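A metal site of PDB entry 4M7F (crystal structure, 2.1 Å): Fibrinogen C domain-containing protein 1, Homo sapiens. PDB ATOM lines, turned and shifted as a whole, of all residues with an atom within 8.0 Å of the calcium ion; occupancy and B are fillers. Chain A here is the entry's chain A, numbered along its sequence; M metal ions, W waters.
The calcium ion is bound by OD2 of Asp 158, OD2 of Asp 160, O of Asn 164, water W1, water W2, O of Ser 162 and OD1 of Asp 158.
The side-chain amide oxygen (OD1) of Asn 178 sits close to the side-chain hydroxyl (OG) of Ser 162.
The backbone NH (N) of Cys 166 lies within hydrogen-bond range of the side-chain carboxylate (OD1) of Asp 160 (2.9 Å).
N of Asp 160 lies within hydrogen-bond range of OG1 of Thr 153 (3.2 Å).
The side-chain sulfur (SG) of Cys 166 forms a disulfide with the side-chain sulfur (SG) of Cys 179 (2.0 Å).
The backbone NH of Asn 164 sits close to the side-chain hydroxyl of Ser 162, at 3.2 Å.
Within 4 Å of the calcium ion: Asp 158, Asp 160, Ser 162 and Asn 164.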
ATOM      1  N   THR A 153       8.996 -20.978  27.005  1.00  0.00           N
ATOM      2  CA  THR A 153      10.071 -21.963  26.911  1.00  0.00           C
ATOM      3  C   THR A 153      10.032 -23.004  28.029  1.00  0.00           C
ATOM      4  O   THR A 153       9.858 -22.675  29.204  1.00  0.00           O
ATOM      5  CB  THR A 153      11.454 -21.258  26.930  1.00  0.00           C
ATOM      6  OG1 THR A 153      11.734 -20.735  25.629  1.00  0.00           O
ATOM      7  CG2 THR A 153      12.549 -22.228  27.339  1.00  0.00           C
ATOM      8  N   ARG A 157      11.954 -27.430  24.964  1.00  0.00           N
ATOM      9  CA  ARG A 157      11.624 -26.597  23.802  1.00  0.00           C
ATOM     10  C   ARG A 157      12.086 -25.163  24.061  1.00  0.00           C
ATOM     11  O   ARG A 157      11.361 -24.350  24.645  1.00  0.00           O
ATOM     12  CB  ARG A 157      10.113 -26.629  23.521  1.00  0.00           C
ATOM     13  CG  ARG A 157       9.734 -26.105  22.127  1.00  0.00           C
ATOM     14  CD  ARG A 157       8.240 -26.276  21.866  1.00  0.00           C
ATOM     15  NE  ARG A 157       7.844 -25.934  20.497  1.00  0.00           N
ATOM     16  CZ  ARG A 157       7.771 -24.696  20.011  1.00  0.00           C
ATOM     17  NH1 ARG A 157       8.064 -23.656  20.790  1.00  0.00           N
ATOM     18  NH2 ARG A 157       7.410 -24.492  18.759  1.00  0.00           N
ATOM     19  N   ASP A 158      13.306 -24.884  23.598  1.00  0.00           N
ATOM     20  CA  ASP A 158      13.961 -23.588  23.770  1.00  0.00           C
ATOM     21  C   ASP A 158      13.606 -22.526  22.743  1.00  0.00           C
ATOM     22  O   ASP A 158      13.946 -22.657  21.565  1.00  0.00           O
ATOM     23  CB  ASP A 158      15.483 -23.811  23.749  1.00  0.00           C
ATOM     24  CG  ASP A 158      16.273 -22.593  24.175  1.00  0.00           C
ATOM     25  OD1 ASP A 158      15.833 -21.445  23.905  1.00  0.00           O
ATOM     26  OD2 ASP A 158      17.355 -22.777  24.773  1.00  0.00           O
ATOM     27  N   SER A 159      12.955 -21.457  23.185  1.00  0.00           N
ATOM     28  CA  SER A 159      12.585 -20.337  22.312  1.00  0.00           C
ATOM     29  C   SER A 159      12.998 -19.024  22.992  1.00  0.00           C
ATOM     30  O   SER A 159      12.472 -17.966  22.673  1.00  0.00           O
ATOM     31  CB  SER A 159      11.063 -20.290  22.066  1.00  0.00           C
ATOM     32  OG  SER A 159      10.607 -21.399  21.299  1.00  0.00           O
ATOM     33  N   ASP A 160      13.940 -19.109  23.923  1.00  0.00           N
ATOM     34  CA  ASP A 160      14.382 -17.917  24.651  1.00  0.00           C
ATOM     35  C   ASP A 160      15.537 -17.187  23.967  1.00  0.00           C
ATOM     36  O   ASP A 160      15.958 -17.554  22.870  1.00  0.00           O
ATOM     37  CB  ASP A 160      14.779 -18.306  26.079  1.00  0.00           C
ATOM     38  CG  ASP A 160      16.004 -19.204  26.136  1.00  0.00           C
ATOM     39  OD1 ASP A 160      16.009 -20.167  26.924  1.00  0.00           O
ATOM     40  OD2 ASP A 160      16.978 -18.922  25.403  1.00  0.00           O
ATOM     41  N   HIS A 161      16.038 -16.146  24.621  1.00  0.00           N
ATOM     42  CA  HIS A 161      17.143 -15.378  24.071  1.00  0.00           C
ATOM     43  C   HIS A 161      18.458 -15.632  24.787  1.00  0.00           C
ATOM     44  O   HIS A 161      19.315 -14.750  24.880  1.00  0.00           O
ATOM     45  CB  HIS A 161      16.816 -13.877  24.106  1.00  0.00           C
ATOM     46  CG  HIS A 161      15.774 -13.466  23.111  1.00  0.00           C
ATOM     47  ND1 HIS A 161      15.411 -12.148  22.915  1.00  0.00           N
ATOM     48  CD2 HIS A 161      15.043 -14.189  22.228  1.00  0.00           C
ATOM     49  CE1 HIS A 161      14.492 -12.082  21.970  1.00  0.00           C
ATOM     50  NE2 HIS A 161      14.255 -13.312  21.537  1.00  0.00           N
ATOM     51  N   SER A 162      18.615 -16.845  25.301  1.00  0.00           N
ATOM     52  CA  SER A 162      19.844 -17.211  25.993  1.00  0.00           C
ATOM     53  C   SER A 162      20.590 -18.273  25.205  1.00  0.00           C
ATOM     54  O   SER A 162      19.978 -19.022  24.431  1.00  0.00           O
ATOM     55  CB  SER A 162      19.506 -17.749  27.389  1.00  0.00           C
ATOM     56  OG  SER A 162      20.674 -18.240  28.024  1.00  0.00           O
ATOM     57  N   GLU A 163      21.906 -18.336  25.391  1.00  0.00           N
ATOM     58  CA  GLU A 163      22.738 -19.316  24.702  1.00  0.00           C
ATOM     59  C   GLU A 163      22.407 -20.708  25.210  1.00  0.00           C
ATOM     60  O   GLU A 163      22.713 -21.716  24.560  1.00  0.00           O
ATOM     61  CB  GLU A 163      24.220 -19.001  24.955  1.00  0.00           C
ATOM     62  CG  GLU A 163      24.568 -17.525  24.866  1.00  0.00           C
ATOM     63  CD  GLU A 163      24.022 -16.729  26.046  1.00  0.00           C
ATOM     64  OE1 GLU A 163      24.515 -16.929  27.187  1.00  0.00           O
ATOM     65  OE2 GLU A 163      23.101 -15.905  25.852  1.00  0.00           O
ATOM     66  N   ASN A 164      21.791 -20.768  26.380  1.00  0.00           N
ATOM     67  CA  ASN A 164      21.399 -22.050  26.949  1.00  0.00           C
ATOM     68  C   ASN A 164      19.879 -22.085  27.067  1.00  0.00           C
ATOM     69  O   ASN A 164      19.191 -21.211  26.523  1.00  0.00           O
ATOM     70  CB  ASN A 164      22.051 -22.259  28.316  1.00  0.00           C
ATOM     71  CG  ASN A 164      21.692 -21.186  29.319  1.00  0.00           C
ATOM     72  OD1 ASN A 164      20.537 -21.046  29.703  1.00  0.00           O
ATOM     73  ND2 ASN A 164      22.700 -20.423  29.749  1.00  0.00           N
ATOM     74  N   ASN A 165      19.364 -23.087  27.755  1.00  0.00           N
ATOM     75  CA  ASN A 165      17.923 -23.215  27.936  1.00  0.00           C
ATOM     76  C   ASN A 165      17.544 -22.659  29.299  1.00  0.00           C
ATOM     77  O   ASN A 165      17.800 -23.277  30.332  1.00  0.00           O
ATOM     78  CB  ASN A 165      17.497 -24.685  27.839  1.00  0.00           C
ATOM     79  CG  ASN A 165      15.992 -24.853  27.905  1.00  0.00           C
ATOM     80  OD1 ASN A 165      15.338 -24.322  28.797  1.00  0.00           O
ATOM     81  ND2 ASN A 165      15.435 -25.603  26.958  1.00  0.00           N
ATOM     82  N   CYS A 166      16.933 -21.482  29.305  1.00  0.00           N
ATOM     83  CA  CYS A 166      16.531 -20.826  30.540  1.00  0.00           C
ATOM     84  C   CYS A 166      15.657 -21.697  31.452  1.00  0.00           C
ATOM     85  O   CYS A 166      15.836 -21.710  32.672  1.00  0.00           O
ATOM     86  CB  CYS A 166      15.794 -19.530  30.233  1.00  0.00           C
ATOM     87  SG  CYS A 166      16.768 -18.166  29.501  1.00  0.00           S
ATOM     88  N   ALA A 167      14.697 -22.417  30.872  1.00  0.00           N
ATOM     89  CA  ALA A 167      13.800 -23.271  31.651  1.00  0.00           C
ATOM     90  C   ALA A 167      14.586 -24.310  32.447  1.00  0.00           C
ATOM     91  O   ALA A 167      14.319 -24.525  33.627  1.00  0.00           O
ATOM     92  CB  ALA A 167      12.800 -23.958  30.728  1.00  0.00           C
ATOM     93  N   TYR A 176      10.636 -16.766  29.028  1.00  0.00           N
ATOM     94  CA  TYR A 176      12.019 -16.375  29.231  1.00  0.00           C
ATOM     95  C   TYR A 176      12.664 -15.505  28.156  1.00  0.00           C
ATOM     96  O   TYR A 176      12.405 -15.664  26.967  1.00  0.00           O
ATOM     97  CB  TYR A 176      12.884 -17.630  29.397  1.00  0.00           C
ATOM     98  CG  TYR A 176      12.609 -18.448  30.635  1.00  0.00           C
ATOM     99  CD1 TYR A 176      12.795 -17.913  31.905  1.00  0.00           C
ATOM    100  CD2 TYR A 176      12.202 -19.779  30.531  1.00  0.00           C
ATOM    101  CE1 TYR A 176      12.577 -18.682  33.059  1.00  0.00           C
ATOM    102  CE2 TYR A 176      11.981 -20.550  31.663  1.00  0.00           C
ATOM    103  CZ  TYR A 176      12.173 -20.004  32.927  1.00  0.00           C
ATOM    104  OH  TYR A 176      11.975 -20.773  34.052  1.00  0.00           O
ATOM    105  N   ARG A 177      13.500 -14.580  28.609  1.00  0.00           N
ATOM    106  CA  ARG A 177      14.248 -13.709  27.693  1.00  0.00           C
ATOM    107  C   ARG A 177      15.686 -14.192  27.874  1.00  0.00           C
ATOM    108  O   ARG A 177      16.125 -15.122  27.200  1.00  0.00           O
ATOM    109  CB  ARG A 177      14.103 -12.233  28.090  1.00  0.00           C
ATOM    110  CG  ARG A 177      14.875 -11.277  27.172  1.00  0.00           C
ATOM    111  CD  ARG A 177      14.617  -9.812  27.511  1.00  0.00           C
ATOM    112  NE  ARG A 177      13.261  -9.387  27.172  1.00  0.00           N
ATOM    113  CZ  ARG A 177      12.840  -9.108  25.938  1.00  0.00           C
ATOM    114  NH1 ARG A 177      13.673  -9.192  24.913  1.00  0.00           N
ATOM    115  NH2 ARG A 177      11.581  -8.733  25.741  1.00  0.00           N
ATOM    116  N   ASN A 178      16.405 -13.585  28.825  1.00  0.00           N
ATOM    117  CA  ASN A 178      17.786 -13.995  29.087  1.00  0.00           C
ATOM    118  C   ASN A 178      18.263 -13.591  30.484  1.00  0.00           C
ATOM    119  O   ASN A 178      19.203 -12.812  30.626  1.00  0.00           O
ATOM    120  CB  ASN A 178      18.711 -13.405  28.005  1.00  0.00           C
ATOM    121  CG  ASN A 178      20.144 -13.835  28.181  1.00  0.00           C
ATOM    122  OD1 ASN A 178      20.421 -14.994  28.503  1.00  0.00           O
ATOM    123  ND2 ASN A 178      21.077 -12.919  27.945  1.00  0.00           N
ATOM    124  N   CYS A 179      17.640 -14.145  31.526  1.00  0.00           N
ATOM    125  CA  CYS A 179      16.546 -15.098  31.373  1.00  0.00           C
ATOM    126  C   CYS A 179      15.222 -14.628  31.972  1.00  0.00           C
ATOM    127  O   CYS A 179      14.180 -14.736  31.316  1.00  0.00           O
ATOM    128  CB  CYS A 179      16.914 -16.441  32.005  1.00  0.00           C
ATOM    129  SG  CYS A 179      17.975 -17.550  31.025  1.00  0.00           S
HETATM  130 CA    CA M   1      18.172 -20.674  24.504  1.00  0.00          CA
HETATM  131  O   HOH W   1      19.597 -21.733  22.914  1.00  0.00           O
HETATM  132  O   HOH W   2      17.743 -19.588  22.357  1.00  0.00           O
